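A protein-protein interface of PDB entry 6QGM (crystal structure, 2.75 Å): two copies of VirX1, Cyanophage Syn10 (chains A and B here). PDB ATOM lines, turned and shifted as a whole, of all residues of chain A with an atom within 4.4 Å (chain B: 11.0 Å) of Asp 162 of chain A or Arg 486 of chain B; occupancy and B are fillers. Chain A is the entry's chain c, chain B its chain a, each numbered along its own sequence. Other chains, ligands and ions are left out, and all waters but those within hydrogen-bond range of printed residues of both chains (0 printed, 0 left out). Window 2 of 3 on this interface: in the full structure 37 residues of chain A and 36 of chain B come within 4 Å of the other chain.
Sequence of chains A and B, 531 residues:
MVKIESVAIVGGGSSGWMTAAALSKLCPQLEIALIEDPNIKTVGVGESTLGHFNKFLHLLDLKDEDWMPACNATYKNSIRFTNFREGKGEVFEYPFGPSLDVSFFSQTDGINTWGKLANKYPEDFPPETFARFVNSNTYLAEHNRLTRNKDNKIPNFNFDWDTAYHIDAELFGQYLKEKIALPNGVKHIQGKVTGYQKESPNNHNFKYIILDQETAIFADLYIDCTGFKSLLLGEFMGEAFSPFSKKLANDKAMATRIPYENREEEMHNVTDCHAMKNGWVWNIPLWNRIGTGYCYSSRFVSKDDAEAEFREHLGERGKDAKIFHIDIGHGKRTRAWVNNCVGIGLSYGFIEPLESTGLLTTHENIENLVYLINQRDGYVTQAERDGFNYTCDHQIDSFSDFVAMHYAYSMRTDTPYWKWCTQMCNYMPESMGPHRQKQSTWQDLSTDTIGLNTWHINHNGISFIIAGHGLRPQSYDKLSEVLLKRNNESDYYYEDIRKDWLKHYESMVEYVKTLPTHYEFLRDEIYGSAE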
ATOM      1  N   PHE A  96     -23.175  -5.081 -13.413  1.00  0.00           N
ATOM      2  CA  PHE A  96     -22.893  -4.553 -12.050  1.00  0.00           C
ATOM      3  C   PHE A  96     -23.682  -3.272 -11.807  1.00  0.00           C
ATOM      4  O   PHE A  96     -23.803  -2.445 -12.729  1.00  0.00           O
ATOM      5  CB  PHE A  96     -21.398  -4.323 -11.838  1.00  0.00           C
ATOM      6  CG  PHE A  96     -20.644  -5.598 -11.592  1.00  0.00           C
ATOM      7  CD1 PHE A  96     -20.976  -6.422 -10.521  1.00  0.00           C
ATOM      8  CD2 PHE A  96     -19.649  -6.009 -12.466  1.00  0.00           C
ATOM      9  CE1 PHE A  96     -20.291  -7.602 -10.303  1.00  0.00           C
ATOM     10  CE2 PHE A  96     -18.973  -7.201 -12.256  1.00  0.00           C
ATOM     11  CZ  PHE A  96     -19.294  -7.988 -11.175  1.00  0.00           C
ATOM     12  N   GLY A  97     -24.205  -3.119 -10.593  1.00  0.00           N
ATOM     13  CA  GLY A  97     -25.033  -1.957 -10.229  1.00  0.00           C
ATOM     14  C   GLY A  97     -25.463  -1.990  -8.769  1.00  0.00           C
ATOM     15  O   GLY A  97     -25.791  -3.034  -8.236  1.00  0.00           O
ATOM     16  N   PRO A  98     -25.529  -0.826  -8.097  1.00  0.00           N
ATOM     17  CA  PRO A  98     -25.844  -0.783  -6.674  1.00  0.00           C
ATOM     18  C   PRO A  98     -27.307  -1.209  -6.497  1.00  0.00           C
ATOM     19  O   PRO A  98     -27.595  -1.957  -5.600  1.00  0.00           O
ATOM     20  CB  PRO A  98     -25.628   0.703  -6.314  1.00  0.00           C
ATOM     21  CG  PRO A  98     -25.941   1.454  -7.603  1.00  0.00           C
ATOM     22  CD  PRO A  98     -25.458   0.522  -8.699  1.00  0.00           C
ATOM     23  N   ASN A 137     -25.185   0.102 -17.339  1.00  0.00           N
ATOM     24  CA  ASN A 137     -23.874  -0.593 -17.364  1.00  0.00           C
ATOM     25  C   ASN A 137     -23.960  -1.658 -18.462  1.00  0.00           C
ATOM     26  O   ASN A 137     -22.963  -1.860 -19.157  1.00  0.00           O
ATOM     27  CB  ASN A 137     -23.503  -1.148 -15.989  1.00  0.00           C
ATOM     28  CG  ASN A 137     -22.017  -1.364 -15.796  1.00  0.00           C
ATOM     29  OD1 ASN A 137     -21.231  -1.072 -16.693  1.00  0.00           O
ATOM     30  ND2 ASN A 137     -21.624  -1.865 -14.629  1.00  0.00           N
ATOM     31  N   ASN A 156     -26.970   5.915 -13.377  1.00  0.00           N
ATOM     32  CA  ASN A 156     -26.878   4.982 -12.217  1.00  0.00           C
ATOM     33  C   ASN A 156     -25.648   4.069 -12.341  1.00  0.00           C
ATOM     34  O   ASN A 156     -25.682   2.976 -11.782  1.00  0.00           O
ATOM     35  CB  ASN A 156     -28.164   4.165 -12.057  1.00  0.00           C
ATOM     36  CG  ASN A 156     -28.458   3.853 -10.605  1.00  0.00           C
ATOM     37  OD1 ASN A 156     -28.413   4.765  -9.781  1.00  0.00           O
ATOM     38  ND2 ASN A 156     -28.736   2.592 -10.278  1.00  0.00           N
ATOM     39  N   PHE A 157     -24.589   4.527 -13.014  1.00  0.00           N
ATOM     40  CA  PHE A 157     -23.287   3.827 -13.174  1.00  0.00           C
ATOM     41  C   PHE A 157     -22.186   4.669 -12.534  1.00  0.00           C
ATOM     42  O   PHE A 157     -22.068   5.838 -12.880  1.00  0.00           O
ATOM     43  CB  PHE A 157     -22.959   3.610 -14.652  1.00  0.00           C
ATOM     44  CG  PHE A 157     -21.565   3.095 -14.917  1.00  0.00           C
ATOM     45  CD1 PHE A 157     -21.195   1.820 -14.517  1.00  0.00           C
ATOM     46  CD2 PHE A 157     -20.625   3.887 -15.560  1.00  0.00           C
ATOM     47  CE1 PHE A 157     -19.917   1.344 -14.762  1.00  0.00           C
ATOM     48  CE2 PHE A 157     -19.344   3.416 -15.799  1.00  0.00           C
ATOM     49  CZ  PHE A 157     -18.993   2.140 -15.403  1.00  0.00           C
ATOM     50  N   ASN A 158     -21.410   4.067 -11.640  1.00  0.00           N
ATOM     51  CA  ASN A 158     -20.271   4.693 -10.917  1.00  0.00           C
ATOM     52  C   ASN A 158     -19.020   3.875 -11.252  1.00  0.00           C
ATOM     53  O   ASN A 158     -18.891   2.767 -10.722  1.00  0.00           O
ATOM     54  CB  ASN A 158     -20.617   4.778  -9.427  1.00  0.00           C
ATOM     55  CG  ASN A 158     -19.483   5.113  -8.504  1.00  0.00           C
ATOM     56  OD1 ASN A 158     -18.310   4.973  -8.844  1.00  0.00           O
ATOM     57  ND2 ASN A 158     -19.863   5.438  -7.287  1.00  0.00           N
ATOM     58  N   PHE A 159     -18.138   4.400 -12.102  1.00  0.00           N
ATOM     59  CA  PHE A 159     -16.955   3.689 -12.661  1.00  0.00           C
ATOM     60  C   PHE A 159     -16.214   2.947 -11.547  1.00  0.00           C
ATOM     61  O   PHE A 159     -16.035   1.718 -11.696  1.00  0.00           O
ATOM     62  CB  PHE A 159     -16.012   4.649 -13.393  1.00  0.00           C
ATOM     63  CG  PHE A 159     -14.736   4.003 -13.875  1.00  0.00           C
ATOM     64  CD1 PHE A 159     -14.745   3.168 -14.983  1.00  0.00           C
ATOM     65  CD2 PHE A 159     -13.542   4.183 -13.193  1.00  0.00           C
ATOM     66  CE1 PHE A 159     -13.590   2.526 -15.402  1.00  0.00           C
ATOM     67  CE2 PHE A 159     -12.382   3.555 -13.618  1.00  0.00           C
ATOM     68  CZ  PHE A 159     -12.406   2.730 -14.719  1.00  0.00           C
ATOM     69  N   ASP A 160     -15.805   3.645 -10.474  1.00  0.00           N
ATOM     70  CA  ASP A 160     -15.007   3.071  -9.357  1.00  0.00           C
ATOM     71  C   ASP A 160     -15.650   1.789  -8.818  1.00  0.00           C
ATOM     72  O   ASP A 160     -14.916   0.802  -8.659  1.00  0.00           O
ATOM     73  CB  ASP A 160     -14.866   4.062  -8.207  1.00  0.00           C
ATOM     74  CG  ASP A 160     -13.603   4.877  -8.219  1.00  0.00           C
ATOM     75  OD1 ASP A 160     -13.037   5.042  -9.323  1.00  0.00           O
ATOM     76  OD2 ASP A 160     -13.198   5.304  -7.110  1.00  0.00           O
ATOM     77  N   TRP A 161     -16.956   1.818  -8.531  1.00  0.00           N
ATOM     78  CA  TRP A 161     -17.652   0.805  -7.695  1.00  0.00           C
ATOM     79  C   TRP A 161     -18.482  -0.176  -8.529  1.00  0.00           C
ATOM     80  O   TRP A 161     -18.695  -1.293  -8.030  1.00  0.00           O
ATOM     81  CB  TRP A 161     -18.488   1.523  -6.635  1.00  0.00           C
ATOM     82  CG  TRP A 161     -17.612   2.169  -5.609  1.00  0.00           C
ATOM     83  CD1 TRP A 161     -17.106   3.433  -5.602  1.00  0.00           C
ATOM     84  CD2 TRP A 161     -17.053   1.522  -4.457  1.00  0.00           C
ATOM     85  NE1 TRP A 161     -16.317   3.637  -4.507  1.00  0.00           N
ATOM     86  CE2 TRP A 161     -16.216   2.466  -3.810  1.00  0.00           C
ATOM     87  CE3 TRP A 161     -17.183   0.232  -3.920  1.00  0.00           C
ATOM     88  CZ2 TRP A 161     -15.589   2.175  -2.600  1.00  0.00           C
ATOM     89  CZ3 TRP A 161     -16.520  -0.063  -2.755  1.00  0.00           C
ATOM     90  CH2 TRP A 161     -15.736   0.896  -2.107  1.00  0.00           C
ATOM     91  N   ASP A 162     -18.942   0.217  -9.725  1.00  0.00           N
ATOM     92  CA  ASP A 162     -19.795  -0.614 -10.625  1.00  0.00           C
ATOM     93  C   ASP A 162     -18.938  -1.265 -11.716  1.00  0.00           C
ATOM     94  O   ASP A 162     -19.512  -1.942 -12.584  1.00  0.00           O
ATOM     95  CB  ASP A 162     -20.908   0.213 -11.274  1.00  0.00           C
ATOM     96  CG  ASP A 162     -21.979   0.660 -10.292  1.00  0.00           C
ATOM     97  OD1 ASP A 162     -22.107   0.003  -9.237  1.00  0.00           O
ATOM     98  OD2 ASP A 162     -22.669   1.667 -10.571  1.00  0.00           O
ATOM     99  N   THR A 163     -17.622  -1.053 -11.699  1.00  0.00           N
ATOM    100  CA  THR A 163     -16.667  -1.783 -12.567  1.00  0.00           C
ATOM    101  C   THR A 163     -15.758  -2.619 -11.674  1.00  0.00           C
ATOM    102  O   THR A 163     -15.119  -2.039 -10.769  1.00  0.00           O
ATOM    103  CB  THR A 163     -15.853  -0.847 -13.464  1.00  0.00           C
ATOM    104  OG1 THR A 163     -16.751   0.029 -14.144  1.00  0.00           O
ATOM    105  CG2 THR A 163     -15.027  -1.602 -14.482  1.00  0.00           C
ATOM    106  N   ALA A 164     -15.759  -3.929 -11.904  1.00  0.00           N
ATOM    107  CA  ALA A 164     -14.856  -4.921 -11.281  1.00  0.00           C
ATOM    108  C   ALA A 164     -13.753  -5.274 -12.291  1.00  0.00           C
ATOM    109  O   ALA A 164     -13.560  -4.489 -13.256  1.00  0.00           O
ATOM    110  CB  ALA A 164     -15.650  -6.142 -10.877  1.00  0.00           C
ATOM    111  N   LYS B 478     -11.581   3.447   9.104  1.00  0.00           N
ATOM    112  CA  LYS B 478     -11.236   3.245   7.669  1.00  0.00           C
ATOM    113  C   LYS B 478     -12.399   2.531   6.973  1.00  0.00           C
ATOM    114  O   LYS B 478     -12.561   2.724   5.753  1.00  0.00           O
ATOM    115  CB  LYS B 478      -9.901   2.514   7.591  1.00  0.00           C
ATOM    116  CG  LYS B 478      -9.459   2.014   6.225  1.00  0.00           C
ATOM    117  CD  LYS B 478      -9.276   3.098   5.232  1.00  0.00           C
ATOM    118  CE  LYS B 478      -8.802   2.546   3.901  1.00  0.00           C
ATOM    119  NZ  LYS B 478      -7.842   3.440   3.193  1.00  0.00           N
ATOM    120  N   LEU B 479     -13.169   1.747   7.732  1.00  0.00           N
ATOM    121  CA  LEU B 479     -14.336   0.963   7.247  1.00  0.00           C
ATOM    122  C   LEU B 479     -15.488   1.904   6.880  1.00  0.00           C
ATOM    123  O   LEU B 479     -16.054   1.750   5.766  1.00  0.00           O
ATOM    124  CB  LEU B 479     -14.704  -0.012   8.365  1.00  0.00           C
ATOM    125  CG  LEU B 479     -15.855  -0.950   8.060  1.00  0.00           C
ATOM    126  CD1 LEU B 479     -15.669  -1.597   6.689  1.00  0.00           C
ATOM    127  CD2 LEU B 479     -15.962  -1.994   9.167  1.00  0.00           C
ATOM    128  N   SER B 480     -15.799   2.827   7.793  1.00  0.00           N
ATOM    129  CA  SER B 480     -16.772   3.948   7.624  1.00  0.00           C
ATOM    130  C   SER B 480     -16.395   4.791   6.395  1.00  0.00           C
ATOM    131  O   SER B 480     -17.270   5.021   5.528  1.00  0.00           O
ATOM    132  CB  SER B 480     -16.834   4.817   8.868  1.00  0.00           C
ATOM    133  OG  SER B 480     -16.867   4.018  10.060  1.00  0.00           O
ATOM    134  N   GLU B 481     -15.131   5.238   6.342  1.00  0.00           N
ATOM    135  CA  GLU B 481     -14.522   6.072   5.266  1.00  0.00           C
ATOM    136  C   GLU B 481     -14.862   5.485   3.896  1.00  0.00           C
ATOM    137  O   GLU B 481     -15.293   6.270   3.017  1.00  0.00           O
ATOM    138  CB  GLU B 481     -13.004   6.080   5.449  1.00  0.00           C
ATOM    139  CG  GLU B 481     -12.220   7.251   4.913  1.00  0.00           C
ATOM    140  CD  GLU B 481     -10.734   6.923   4.794  1.00  0.00           C
ATOM    141  OE1 GLU B 481     -10.031   6.902   5.841  1.00  0.00           O
ATOM    142  OE2 GLU B 481     -10.268   6.687   3.656  1.00  0.00           O
ATOM    143  N   VAL B 482     -14.665   4.167   3.742  1.00  0.00           N
ATOM    144  CA  VAL B 482     -14.735   3.443   2.444  1.00  0.00           C
ATOM    145  C   VAL B 482     -16.185   3.404   1.956  1.00  0.00           C
ATOM    146  O   VAL B 482     -16.370   3.464   0.714  1.00  0.00           O
ATOM    147  CB  VAL B 482     -14.109   2.038   2.567  1.00  0.00           C
ATOM    148  CG1 VAL B 482     -14.724   1.011   1.622  1.00  0.00           C
ATOM    149  CG2 VAL B 482     -12.612   2.102   2.350  1.00  0.00           C
ATOM    150  N   LEU B 483     -17.165   3.346   2.872  1.00  0.00           N
ATOM    151  CA  LEU B 483     -18.609   3.300   2.513  1.00  0.00           C
ATOM    152  C   LEU B 483     -19.106   4.688   2.057  1.00  0.00           C
ATOM    153  O   LEU B 483     -19.998   4.733   1.182  1.00  0.00           O
ATOM    154  CB  LEU B 483     -19.377   2.708   3.699  1.00  0.00           C
ATOM    155  CG  LEU B 483     -19.013   1.241   3.999  1.00  0.00           C
ATOM    156  CD1 LEU B 483     -19.377   0.807   5.418  1.00  0.00           C
ATOM    157  CD2 LEU B 483     -19.653   0.304   2.969  1.00  0.00           C
ATOM    158  N   LEU B 484     -18.491   5.785   2.507  1.00  0.00           N
ATOM    159  CA  LEU B 484     -18.823   7.175   2.060  1.00  0.00           C
ATOM    160  C   LEU B 484     -18.278   7.437   0.645  1.00  0.00           C
ATOM    161  O   LEU B 484     -18.755   8.417  -0.037  1.00  0.00           O
ATOM    162  CB  LEU B 484     -18.198   8.197   3.006  1.00  0.00           C
ATOM    163  CG  LEU B 484     -18.607   8.133   4.481  1.00  0.00           C
ATOM    164  CD1 LEU B 484     -17.960   9.285   5.248  1.00  0.00           C
ATOM    165  CD2 LEU B 484     -20.129   8.174   4.679  1.00  0.00           C
ATOM    166  N   LYS B 485     -17.266   6.660   0.234  1.00  0.00           N
ATOM    167  CA  LYS B 485     -16.459   6.966  -0.968  1.00  0.00           C
ATOM    168  C   LYS B 485     -17.283   6.763  -2.240  1.00  0.00           C
ATOM    169  O   LYS B 485     -16.919   7.421  -3.217  1.00  0.00           O
ATOM    170  CB  LYS B 485     -15.168   6.141  -0.987  1.00  0.00           C
ATOM    171  CG  LYS B 485     -14.348   6.173  -2.271  1.00  0.00           C
ATOM    172  CD  LYS B 485     -13.676   7.475  -2.626  1.00  0.00           C
ATOM    173  CE  LYS B 485     -13.478   7.587  -4.121  1.00  0.00           C
ATOM    174  NZ  LYS B 485     -12.219   8.300  -4.413  1.00  0.00           N
ATOM    175  N   ARG B 486     -18.335   5.928  -2.245  1.00  0.00           N
ATOM    176  CA  ARG B 486     -19.147   5.697  -3.480  1.00  0.00           C
ATOM    177  C   ARG B 486     -19.632   7.049  -4.029  1.00  0.00           C
ATOM    178  O   ARG B 486     -19.203   7.419  -5.148  1.00  0.00           O
ATOM    179  CB  ARG B 486     -20.342   4.757  -3.280  1.00  0.00           C
ATOM    180  CG  ARG B 486     -21.137   4.543  -4.565  1.00  0.00           C
ATOM    181  CD  ARG B 486     -22.292   3.563  -4.546  1.00  0.00           C
ATOM    182  NE  ARG B 486     -22.377   2.758  -5.771  1.00  0.00           N
ATOM    183  CZ  ARG B 486     -22.817   3.187  -6.961  1.00  0.00           C
ATOM    184  NH1 ARG B 486     -23.234   4.429  -7.120  1.00  0.00           N
ATOM    185  NH2 ARG B 486     -22.824   2.373  -7.998  1.00  0.00           N
ATOM    186  N   ASN B 487     -20.473   7.761  -3.268  1.00  0.00           N
ATOM    187  CA  ASN B 487     -21.164   9.007  -3.702  1.00  0.00           C
ATOM    188  C   ASN B 487     -20.401  10.219  -3.149  1.00  0.00           C
ATOM    189  O   ASN B 487     -21.073  11.188  -2.778  1.00  0.00           O
ATOM    190  CB  ASN B 487     -22.643   9.042  -3.307  1.00  0.00           C
ATOM    191  CG  ASN B 487     -23.217   7.687  -2.957  1.00  0.00           C
ATOM    192  OD1 ASN B 487     -23.547   6.891  -3.833  1.00  0.00           O
ATOM    193  ND2 ASN B 487     -23.516   7.480  -1.683  1.00  0.00           N
ATOM    194  N   ASN B 488     -19.064  10.158  -3.084  1.00  0.00           N
ATOM    195  CA  ASN B 488     -18.141  11.237  -2.621  1.00  0.00           C
ATOM    196  C   ASN B 488     -18.756  11.999  -1.436  1.00  0.00           C
ATOM    197  O   ASN B 488     -18.830  13.251  -1.513  1.00  0.00           O
ATOM    198  CB  ASN B 488     -17.752  12.174  -3.772  1.00  0.00           C
ATOM    199  CG  ASN B 488     -16.599  13.109  -3.447  1.00  0.00           C
ATOM    200  OD1 ASN B 488     -15.954  12.986  -2.409  1.00  0.00           O
ATOM    201  ND2 ASN B 488     -16.323  14.058  -4.330  1.00  0.00           N
ATOM    202  N   GLU B 489     -19.153  11.278  -0.372  1.00  0.00           N
ATOM    203  CA  GLU B 489     -19.795  11.871   0.835  1.00  0.00           C
ATOM    204  C   GLU B 489     -18.754  12.017   1.949  1.00  0.00           C
ATOM    205  O   GLU B 489     -17.634  11.477   1.791  1.00  0.00           O
ATOM    206  CB  GLU B 489     -20.983  11.026   1.282  1.00  0.00           C
ATOM    207  CG  GLU B 489     -21.945  10.750   0.152  1.00  0.00           C
ATOM    208  CD  GLU B 489     -23.375  10.413   0.507  1.00  0.00           C
ATOM    209  OE1 GLU B 489     -23.613  10.106   1.692  1.00  0.00           O
ATOM    210  OE2 GLU B 489     -24.231  10.455  -0.418  1.00  0.00           O
ATOM    211  N   SER B 490     -19.086  12.779   2.992  1.00  0.00           N
ATOM    212  CA  SER B 490     -18.090  13.371   3.925  1.00  0.00           C
ATOM    213  C   SER B 490     -18.537  13.203   5.376  1.00  0.00           C
ATOM    214  O   SER B 490     -19.731  13.295   5.634  1.00  0.00           O
ATOM    215  CB  SER B 490     -17.840  14.811   3.592  1.00  0.00           C
ATOM    216  OG  SER B 490     -17.093  15.409   4.624  1.00  0.00           O
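The backbone carbonyl oxygen (O) of Arg 486 of chain B is in hydrogen-bond range of the side-chain amide nitrogen (ND2) of Asn 158 of chain A (3.0 Å).
The guanidinium group (NH2) of Arg 486 of chain B lies within salt-bridge range of the side-chain carboxylate (OD2) of Asp 162 of chain A, 2.7 Å away.
The side-chain amide oxygen of Asn 158 of chain A lies within hydrogen-bond range of the backbone NH of Trp 161 of chain A.
The backbone NH of Asp 160 of chain A is in hydrogen-bond range of the side-chain amide oxygen of Asn 158 of chain A, at 3.3 Å.
O of Asp 162 of chain A is in hydrogen-bond range of ND2 of Asn 137 of chain A (2.9 Å).
OD2 of Asp 162 of chain A is in hydrogen-bond range of N of Asn 158 of chain A (2.9 Å).
Pro 98 of chain A touches Arg 486 of chain B (CG to NH2, 3.3 Å).
CE of Lys 485 of chain B touches OD2 of Asp 160 of chain A, 3.8 Å away.
Trp 161 of chain A touches Val 482 of chain B (CZ2 to O, 3.6 Å).
Trp 161 of chain A touches Lys 485 of chain B.
NE1 of Trp 161 of chain A touches CA of Arg 486 of chain B (3.6 Å).
Pro 98 of chain A touches just one residue of chain B: Arg 486.
No residue of chain B comes within 4 Å of Asn 156 of chain A.
No residue of chain B comes within 4 Å of Phe 157 of chain A.
Printed residues of chain B within 4 Å of Asp 160 of chain A: Lys 485 (3.8 Å).
Asp 162 of chain A touches just one residue of chain B: Arg 486 (2.7 Å).
No residue of chain B comes within 4 Å of Thr 163 of chain A.
No residue of chain B comes within 4 Å of Ala 164 of chain A.
Glu 481 of chain B touches none of the printed residues of chain A.
Of the printed residues of chain A, Val 482 of chain B touches Trp 161.
Of the printed residues of chain A, Lys 485 of chain B touches Asp 160 (3.8 Å) and Trp 161 (3.9 Å).
Asn 487 of chain B touches none of the printed residues of chain A.
The nearest residue of chain B that does not touch Asp 162 of chain A is Asn 487 of chain B (8.6 Å).
The nearest printed residue of chain A that does not touch Val 482 of chain B is Asp 160 of chain A (8.6 Å).
Hydrophobic or aromatic side chains of chain A that line the printed part of chain B: Pro 98 and Trp 161.
Of the 13 printed residues of chain B, 3 touch a printed residue of chain A.
Among the printed residues, 7 pairs touch across the chains.
Among the printed residues, Asp or Glu carboxylates within 4 Å of a Lys or Arg side-chain nitrogen of the other chain: Asp 162 of chain A with Arg 486 of chain B (2.7 Å).
No position is printed for both chains.
Of the 7 pairs that touch across the chains among the printed residues, none has its exchanged pair printed and touching as well.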
